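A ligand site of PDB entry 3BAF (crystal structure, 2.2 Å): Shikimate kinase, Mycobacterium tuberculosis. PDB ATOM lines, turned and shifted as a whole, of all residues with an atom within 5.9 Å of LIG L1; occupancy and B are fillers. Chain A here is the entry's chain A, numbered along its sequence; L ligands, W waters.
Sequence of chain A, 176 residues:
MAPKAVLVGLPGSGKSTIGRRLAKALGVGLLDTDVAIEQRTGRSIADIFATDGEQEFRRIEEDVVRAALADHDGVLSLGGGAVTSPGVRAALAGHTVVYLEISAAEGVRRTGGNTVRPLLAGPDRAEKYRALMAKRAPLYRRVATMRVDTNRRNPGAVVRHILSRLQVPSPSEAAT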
ATOM      1  N   GLY A   9      10.660  -8.480 -12.372  1.00  0.00           N
ATOM      2  CA  GLY A   9       9.570  -7.814 -11.621  1.00  0.00           C
ATOM      3  C   GLY A   9       8.222  -7.624 -12.364  1.00  0.00           C
ATOM      4  O   GLY A   9       8.126  -7.936 -13.561  1.00  0.00           O
ATOM      5  N   LEU A  10       7.196  -7.073 -11.688  1.00  0.00           N
ATOM      6  CA  LEU A  10       5.813  -6.757 -12.269  1.00  0.00           C
ATOM      7  C   LEU A  10       5.846  -5.643 -13.333  1.00  0.00           C
ATOM      8  O   LEU A  10       6.759  -4.792 -13.284  1.00  0.00           O
ATOM      9  CB  LEU A  10       4.794  -6.305 -11.152  1.00  0.00           C
ATOM     10  CG  LEU A  10       4.385  -7.250  -9.953  1.00  0.00           C
ATOM     11  CD1 LEU A  10       3.737  -6.537  -8.729  1.00  0.00           C
ATOM     12  CD2 LEU A  10       3.469  -8.485 -10.392  1.00  0.00           C
ATOM     13  N   PRO A  11       4.848  -5.599 -14.241  1.00  0.00           N
ATOM     14  CA  PRO A  11       4.651  -4.435 -15.151  1.00  0.00           C
ATOM     15  C   PRO A  11       4.615  -3.083 -14.390  1.00  0.00           C
ATOM     16  O   PRO A  11       4.001  -3.023 -13.304  1.00  0.00           O
ATOM     17  CB  PRO A  11       3.321  -4.754 -15.885  1.00  0.00           C
ATOM     18  CG  PRO A  11       2.682  -5.836 -15.045  1.00  0.00           C
ATOM     19  CD  PRO A  11       3.813  -6.634 -14.450  1.00  0.00           C
ATOM     20  N   GLY A  12       5.345  -2.044 -14.849  1.00  0.00           N
ATOM     21  CA  GLY A  12       5.550  -0.781 -14.086  1.00  0.00           C
ATOM     22  C   GLY A  12       6.613  -0.603 -12.985  1.00  0.00           C
ATOM     23  O   GLY A  12       6.743   0.520 -12.460  1.00  0.00           O
ATOM     24  N   SER A  13       7.325  -1.693 -12.600  1.00  0.00           N
ATOM     25  CA  SER A  13       8.541  -1.617 -11.701  1.00  0.00           C
ATOM     26  C   SER A  13       9.784  -0.862 -12.341  1.00  0.00           C
ATOM     27  O   SER A  13      10.663  -0.454 -11.601  1.00  0.00           O
ATOM     28  CB  SER A  13       8.989  -3.045 -11.142  1.00  0.00           C
ATOM     29  OG  SER A  13       9.311  -3.981 -12.214  1.00  0.00           O
ATOM     30  N   GLY A  14       9.867  -0.709 -13.675  1.00  0.00           N
ATOM     31  CA  GLY A  14      11.011  -0.025 -14.392  1.00  0.00           C
ATOM     32  C   GLY A  14      12.053  -0.862 -15.209  1.00  0.00           C
ATOM     33  O   GLY A  14      13.128  -0.355 -15.584  1.00  0.00           O
ATOM     34  N   LYS A  15      11.801  -2.164 -15.494  1.00  0.00           N
ATOM     35  CA  LYS A  15      12.733  -3.038 -16.341  1.00  0.00           C
ATOM     36  C   LYS A  15      13.272  -2.357 -17.667  1.00  0.00           C
ATOM     37  O   LYS A  15      14.499  -2.374 -17.903  1.00  0.00           O
ATOM     38  CB  LYS A  15      12.099  -4.438 -16.678  1.00  0.00           C
ATOM     39  CG  LYS A  15      11.707  -5.376 -15.462  1.00  0.00           C
ATOM     40  CD  LYS A  15      10.894  -6.746 -15.809  1.00  0.00           C
ATOM     41  CE  LYS A  15       9.589  -6.649 -16.740  1.00  0.00           C
ATOM     42  NZ  LYS A  15       8.377  -5.963 -16.018  1.00  0.00           N
ATOM     43  N   SER A  16      12.431  -1.817 -18.558  1.00  0.00           N
ATOM     44  CA  SER A  16      13.001  -1.175 -19.803  1.00  0.00           C
ATOM     45  C   SER A  16      13.789   0.185 -19.596  1.00  0.00           C
ATOM     46  O   SER A  16      14.754   0.433 -20.325  1.00  0.00           O
ATOM     47  CB  SER A  16      11.940  -0.922 -20.878  1.00  0.00           C
ATOM     48  OG  SER A  16      11.237  -2.111 -21.202  1.00  0.00           O
ATOM     49  N   THR A  17      13.323   1.003 -18.621  1.00  0.00           N
ATOM     50  CA  THR A  17      13.804   2.366 -18.278  1.00  0.00           C
ATOM     51  C   THR A  17      15.152   2.294 -17.563  1.00  0.00           C
ATOM     52  O   THR A  17      16.104   2.945 -18.031  1.00  0.00           O
ATOM     53  CB  THR A  17      12.730   3.223 -17.437  1.00  0.00           C
ATOM     54  OG1 THR A  17      11.527   3.446 -18.243  1.00  0.00           O
ATOM     55  CG2 THR A  17      13.313   4.600 -17.016  1.00  0.00           C
ATOM     56  N   ILE A  18      15.224   1.527 -16.474  1.00  0.00           N
ATOM     57  CA  ILE A  18      16.485   1.242 -15.721  1.00  0.00           C
ATOM     58  C   ILE A  18      17.529   0.471 -16.601  1.00  0.00           C
ATOM     59  O   ILE A  18      18.736   0.798 -16.535  1.00  0.00           O
ATOM     60  CB  ILE A  18      16.232   0.537 -14.315  1.00  0.00           C
ATOM     61  CG1 ILE A  18      15.199   1.279 -13.422  1.00  0.00           C
ATOM     62  CG2 ILE A  18      17.572   0.151 -13.531  1.00  0.00           C
ATOM     63  CD1 ILE A  18      15.619   2.833 -13.032  1.00  0.00           C
ATOM     64  N   ASP A  34      10.951  -8.990 -25.041  1.00  0.00           N
ATOM     65  CA  ASP A  34       9.628  -8.697 -25.722  1.00  0.00           C
ATOM     66  C   ASP A  34       9.777  -8.159 -27.139  1.00  0.00           C
ATOM     67  O   ASP A  34       8.999  -8.541 -28.010  1.00  0.00           O
ATOM     68  CB  ASP A  34       8.713  -7.668 -24.969  1.00  0.00           C
ATOM     69  CG  ASP A  34       8.140  -8.156 -23.611  1.00  0.00           C
ATOM     70  OD1 ASP A  34       7.793  -9.367 -23.498  1.00  0.00           O
ATOM     71  OD2 ASP A  34       8.017  -7.321 -22.665  1.00  0.00           O
ATOM     72  N   LEU A  78      13.982  -9.062 -19.060  1.00  0.00           N
ATOM     73  CA  LEU A  78      12.934 -10.149 -19.218  1.00  0.00           C
ATOM     74  C   LEU A  78      11.406  -9.701 -19.246  1.00  0.00           C
ATOM     75  O   LEU A  78      11.045  -8.776 -18.532  1.00  0.00           O
ATOM     76  CB  LEU A  78      13.150 -11.187 -18.074  1.00  0.00           C
ATOM     77  CG  LEU A  78      14.016 -12.454 -18.258  1.00  0.00           C
ATOM     78  CD1 LEU A  78      15.350 -12.224 -19.120  1.00  0.00           C
ATOM     79  CD2 LEU A  78      14.184 -13.436 -17.027  1.00  0.00           C
ATOM     80  N   GLY A  79      10.513 -10.290 -20.041  1.00  0.00           N
ATOM     81  CA  GLY A  79       9.040 -10.087 -19.837  1.00  0.00           C
ATOM     82  C   GLY A  79       8.477 -10.350 -18.426  1.00  0.00           C
ATOM     83  O   GLY A  79       9.048 -11.138 -17.660  1.00  0.00           O
ATOM     84  N   GLY A  80       7.379  -9.699 -18.029  1.00  0.00           N
ATOM     85  CA  GLY A  80       6.904  -9.809 -16.616  1.00  0.00           C
ATOM     86  C   GLY A  80       6.476 -11.161 -16.017  1.00  0.00           C
ATOM     87  O   GLY A  80       6.610 -11.388 -14.801  1.00  0.00           O
ATOM     88  N   GLU A 106       1.000   2.761  -6.318  1.00  0.00           N
ATOM     89  CA  GLU A 106       1.969   3.413  -7.238  1.00  0.00           C
ATOM     90  C   GLU A 106       2.159   2.629  -8.572  1.00  0.00           C
ATOM     91  O   GLU A 106       2.147   3.252  -9.666  1.00  0.00           O
ATOM     92  CB  GLU A 106       3.294   3.687  -6.464  1.00  0.00           C
ATOM     93  CG  GLU A 106       4.402   4.557  -7.222  1.00  0.00           C
ATOM     94  CD  GLU A 106       3.888   5.948  -7.803  1.00  0.00           C
ATOM     95  OE1 GLU A 106       3.080   6.668  -7.159  1.00  0.00           O
ATOM     96  OE2 GLU A 106       4.259   6.317  -8.934  1.00  0.00           O
ATOM     97  N   ARG A 110       1.537   4.077 -12.465  1.00  0.00           N
ATOM     98  CA  ARG A 110       2.571   4.036 -13.539  1.00  0.00           C
ATOM     99  C   ARG A 110       2.132   3.362 -14.869  1.00  0.00           C
ATOM    100  O   ARG A 110       2.596   3.789 -15.936  1.00  0.00           O
ATOM    101  CB  ARG A 110       3.959   3.514 -13.009  1.00  0.00           C
ATOM    102  CG  ARG A 110       4.803   4.416 -12.056  1.00  0.00           C
ATOM    103  CD  ARG A 110       6.061   3.668 -11.520  1.00  0.00           C
ATOM    104  NE  ARG A 110       6.757   4.270 -10.380  1.00  0.00           N
ATOM    105  CZ  ARG A 110       7.899   3.839  -9.835  1.00  0.00           C
ATOM    106  NH1 ARG A 110       8.514   2.720 -10.250  1.00  0.00           N
ATOM    107  NH2 ARG A 110       8.406   4.456  -8.799  1.00  0.00           N
ATOM    108  N   THR A 111       1.265   2.325 -14.849  1.00  0.00           N
ATOM    109  CA  THR A 111       0.759   1.640 -16.084  1.00  0.00           C
ATOM    110  C   THR A 111      -0.424   2.362 -16.807  1.00  0.00           C
ATOM    111  O   THR A 111      -0.960   1.844 -17.816  1.00  0.00           O
ATOM    112  CB  THR A 111       0.423   0.069 -15.891  1.00  0.00           C
ATOM    113  OG1 THR A 111      -0.605  -0.175 -14.889  1.00  0.00           O
ATOM    114  CG2 THR A 111       1.641  -0.770 -15.472  1.00  0.00           C
ATOM    115  N   ARG A 117      -1.377  -4.408 -22.792  1.00  0.00           N
ATOM    116  CA  ARG A 117      -1.226  -5.503 -21.826  1.00  0.00           C
ATOM    117  C   ARG A 117      -2.452  -6.465 -21.635  1.00  0.00           C
ATOM    118  O   ARG A 117      -3.228  -6.295 -20.680  1.00  0.00           O
ATOM    119  CB  ARG A 117      -0.587  -4.988 -20.522  1.00  0.00           C
ATOM    120  CG  ARG A 117       0.832  -4.409 -20.714  1.00  0.00           C
ATOM    121  CD  ARG A 117       1.449  -4.017 -19.383  1.00  0.00           C
ATOM    122  NE  ARG A 117       2.775  -3.362 -19.406  1.00  0.00           N
ATOM    123  CZ  ARG A 117       3.007  -2.040 -19.331  1.00  0.00           C
ATOM    124  NH1 ARG A 117       2.016  -1.151 -19.321  1.00  0.00           N
ATOM    125  NH2 ARG A 117       4.254  -1.588 -19.335  1.00  0.00           N
ATOM    126  N   THR A 150      12.126   0.591  -5.167  1.00  0.00           N
ATOM    127  CA  THR A 150      11.917   1.742  -6.073  1.00  0.00           C
ATOM    128  C   THR A 150      10.777   2.796  -5.710  1.00  0.00           C
ATOM    129  O   THR A 150      10.492   3.706  -6.536  1.00  0.00           O
ATOM    130  CB  THR A 150      11.739   1.258  -7.547  1.00  0.00           C
ATOM    131  OG1 THR A 150      10.377   0.778  -7.795  1.00  0.00           O
ATOM    132  CG2 THR A 150      12.844   0.174  -7.906  1.00  0.00           C
ATOM    133  N   ARG A 153      12.593   6.497  -4.688  1.00  0.00           N
ATOM    134  CA  ARG A 153      13.924   6.736  -5.296  1.00  0.00           C
ATOM    135  C   ARG A 153      13.626   7.187  -6.744  1.00  0.00           C
ATOM    136  O   ARG A 153      12.825   6.539  -7.417  1.00  0.00           O
ATOM    137  CB  ARG A 153      14.791   5.456  -5.302  1.00  0.00           C
ATOM    138  CG  ARG A 153      15.856   5.294  -4.157  1.00  0.00           C
ATOM    139  CD  ARG A 153      16.742   4.013  -4.302  1.00  0.00           C
ATOM    140  NE  ARG A 153      17.574   3.690  -3.143  1.00  0.00           N
ATOM    141  CZ  ARG A 153      17.387   2.632  -2.329  1.00  0.00           C
ATOM    142  NH1 ARG A 153      16.385   1.780  -2.527  1.00  0.00           N
ATOM    143  NH2 ARG A 153      18.194   2.394  -1.292  1.00  0.00           N
ATOM    144  N   ASN A 154      14.218   8.300  -7.207  1.00  0.00           N
ATOM    145  CA  ASN A 154      14.067   8.698  -8.633  1.00  0.00           C
ATOM    146  C   ASN A 154      14.963   7.797  -9.579  1.00  0.00           C
ATOM    147  O   ASN A 154      15.788   7.077  -9.053  1.00  0.00           O
ATOM    148  CB  ASN A 154      14.244  10.218  -8.832  1.00  0.00           C
ATOM    149  CG  ASN A 154      15.658  10.730  -8.468  1.00  0.00           C
ATOM    150  OD1 ASN A 154      16.681  10.230  -8.975  1.00  0.00           O
ATOM    151  ND2 ASN A 154      15.700  11.752  -7.598  1.00  0.00           N
ATOM    152  N   PRO A 155      14.702   7.730 -10.919  1.00  0.00           N
ATOM    153  CA  PRO A 155      15.513   6.746 -11.723  1.00  0.00           C
ATOM    154  C   PRO A 155      17.092   6.784 -11.710  1.00  0.00           C
ATOM    155  O   PRO A 155      17.722   5.683 -11.648  1.00  0.00           O
ATOM    156  CB  PRO A 155      14.903   6.788 -13.149  1.00  0.00           C
ATOM    157  CG  PRO A 155      13.628   7.728 -13.057  1.00  0.00           C
ATOM    158  CD  PRO A 155      13.664   8.434 -11.710  1.00  0.00           C
ATOM    159  N   VAL A 158      18.241   4.974  -8.386  1.00  0.00           N
ATOM    160  CA  VAL A 158      18.198   3.485  -8.618  1.00  0.00           C
ATOM    161  C   VAL A 158      19.521   2.953  -9.301  1.00  0.00           C
ATOM    162  O   VAL A 158      20.200   2.093  -8.700  1.00  0.00           O
ATOM    163  CB  VAL A 158      16.821   2.917  -9.244  1.00  0.00           C
ATOM    164  CG1 VAL A 158      16.837   1.287  -9.451  1.00  0.00           C
ATOM    165  CG2 VAL A 158      15.520   3.401  -8.432  1.00  0.00           C
HETATM  166  P1  LIG L   1       6.435  -5.037 -18.922  1.00  0.00           P
HETATM  167  O1  LIG L   1       5.319  -4.989 -19.971  1.00  0.00           O
HETATM  168  O2  LIG L   1       7.524  -5.690 -19.785  1.00  0.00           O
HETATM  169  O3  LIG L   1       6.035  -6.042 -17.902  1.00  0.00           O
HETATM  170  P2  LIG L   1       8.259  -2.330 -17.309  1.00  0.00           P
HETATM  171  O4  LIG L   1       8.668  -2.947 -15.963  1.00  0.00           O
HETATM  172  O5  LIG L   1       9.393  -2.513 -18.296  1.00  0.00           O
HETATM  173  N1  LIG L   1       6.842  -3.242 -18.159  1.00  0.00           N
HETATM  174  P3  LIG L   1       8.865   0.680 -17.667  1.00  0.00           P
HETATM  175  O6  LIG L   1      10.350   0.898 -17.707  1.00  0.00           O
HETATM  176  O7  LIG L   1       8.105   0.643 -18.923  1.00  0.00           O
HETATM  177  O8  LIG L   1       8.456  -0.710 -16.820  1.00  0.00           O
HETATM  178  O9  LIG L   1       8.221   1.948 -16.811  1.00  0.00           O
HETATM  179  C1  LIG L   1       6.799   2.341 -16.811  1.00  0.00           C
HETATM  180  C2  LIG L   1       6.577   3.881 -16.637  1.00  0.00           C
HETATM  181  O10 LIG L   1       6.965   4.211 -15.297  1.00  0.00           O
HETATM  182  C3  LIG L   1       7.449   4.757 -17.610  1.00  0.00           C
HETATM  183  O11 LIG L   1       6.868   5.959 -18.243  1.00  0.00           O
HETATM  184  C4  LIG L   1       8.582   5.215 -16.730  1.00  0.00           C
HETATM  185  O12 LIG L   1       8.947   6.512 -17.232  1.00  0.00           O
HETATM  186  C5  LIG L   1       8.028   5.225 -15.290  1.00  0.00           C
HETATM  187  N2  LIG L   1       9.027   5.011 -14.195  1.00  0.00           N
HETATM  188  C6  LIG L   1       9.842   3.872 -14.131  1.00  0.00           C
HETATM  189  N3  LIG L   1      10.635   3.864 -13.018  1.00  0.00           N
HETATM  190  C7  LIG L   1      10.346   5.001 -12.314  1.00  0.00           C
HETATM  191  C8  LIG L   1      10.863   5.633 -11.088  1.00  0.00           C
HETATM  192  N4  LIG L   1      11.842   5.064 -10.314  1.00  0.00           N
HETATM  193  N5  LIG L   1      10.312   6.840 -10.713  1.00  0.00           N
HETATM  194  C9  LIG L   1       9.363   7.486 -11.463  1.00  0.00           C
HETATM  195  N6  LIG L   1       8.837   6.965 -12.572  1.00  0.00           N
HETATM  196  C10 LIG L   1       9.298   5.757 -13.097  1.00  0.00           C
HETATM  197  O1  LG2 L   2       5.570  -9.965 -21.770  1.00  0.00           O
HETATM  198  C1  LG2 L   2       4.504  -9.004 -21.530  1.00  0.00           C
HETATM  199  C2  LG2 L   2       4.555  -8.117 -20.226  1.00  0.00           C
HETATM  200  O2  LG2 L   2       5.894  -7.600 -19.831  1.00  0.00           O
HETATM  201  C3  LG2 L   2       3.649  -8.687 -19.078  1.00  0.00           C
HETATM  202  C4  LG2 L   2       3.171  -9.970 -19.075  1.00  0.00           C
HETATM  203  C5  LG2 L   2       2.807 -10.627 -17.948  1.00  0.00           C
HETATM  204  O3  LG2 L   2       2.479 -11.875 -18.062  1.00  0.00           O
HETATM  205  O4  LG2 L   2       2.804 -10.040 -16.799  1.00  0.00           O
HETATM  206  C6  LG2 L   2       3.130 -10.632 -20.259  1.00  0.00           C
HETATM  207  C7  LG2 L   2       3.198  -9.824 -21.565  1.00  0.00           C
HETATM  208  O5  LG2 L   2       2.064  -8.957 -21.865  1.00  0.00           O
HETATM  209  O   HOH W   1      11.168   7.870 -15.634  1.00  0.00           O
HETATM  210  O   HOH W   2      10.167   8.110  -7.661  1.00  0.00           O
HETATM  211  O   HOH W   3       9.438  -3.916 -20.456  1.00  0.00           O
HETATM  212  O   HOH W   4       7.731  -1.795 -20.783  1.00  0.00           O
HETATM  213  O   HOH W   5       4.525  -4.881 -22.657  1.00  0.00           O
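An oxygen (O2) of LG2 L2 lies within hydrogen-bond range of an oxygen (O3) of LIG L1, 2.5 Å away.
Water W3 lies within hydrogen-bond range of O5 of LIG L1 (2.6 Å) and OG of Ser 16 (2.7 Å). Water W2 lies within hydrogen-bond range of the backbone carbonyl oxygen (O) of Arg 153 (3.1 Å) and a nitrogen (N5) of LIG L1 (3.3 Å).
OD2 of Asp 34 sits close to O2 of LIG L1. Residues that only touch LIG L1: Leu 10, Pro 11, Gly 12, Ser 13, Gly 80, Arg 110 and Pro 155. Along chain A the residues within 4 Å of LIG L1 span positions 10 to 155. The nearest printed residue that does not touch LIG L1 is Asn 154 (4.2 Å).
N of Ser 16 lies within hydrogen-bond range of O5 of LIG L1. The backbone NH (N) of Lys 15 is in hydrogen-bond range of an oxygen (O4) of LIG L1, at 3.3 Å. OG1 of Thr 17 is in hydrogen-bond range of O6 of LIG L1 (2.9 Å). The backbone NH (N) of Gly 14 sits at hydrogen-bond distance from an oxygen (O4) of LIG L1 (3.4 Å). OG of Ser 16 sits at hydrogen-bond distance from O5 of LIG L1, 3.5 Å away. The backbone NH (N) of Gly 80 is in hydrogen-bond range of an oxygen (O2) of LG2 L2. O of Arg 153 lies within hydrogen-bond range of N4 of LIG L1 (3.4 Å). An oxygen (O6) of LIG L1 is in hydrogen-bond range of the backbone NH (N) of Thr 17 (3.1 Å). OD1 of Asp 34 lies within hydrogen-bond range of O1 of LG2 L2. The guanidinium group (NE) of Arg 117 is in salt-bridge range of an oxygen (O1) of LIG L1, 3.1 Å away. O3 of LIG L1 is in salt-bridge range of NZ of Lys 15, at 3.0 Å.
O of Gly 9 lies within hydrogen-bond range of NZ of Lys 15 (3.2 Å). The guanidinium group of Arg 110 sits at hydrogen-bond distance from the backbone carbonyl oxygen of Thr 150 (3.2 Å). The backbone carbonyl oxygen of Leu 10 is in hydrogen-bond range of the side-chain hydroxyl of Ser 13, 2.9 Å away. The side-chain amino group (NZ) of Lys 15 sits at hydrogen-bond distance from the backbone carbonyl oxygen (O) of Leu 10, at 3.4 Å. The guanidinium group (NE) of Arg 110 lies within salt-bridge range of the side-chain carboxylate (OE2) of Glu 106 (3.5 Å).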
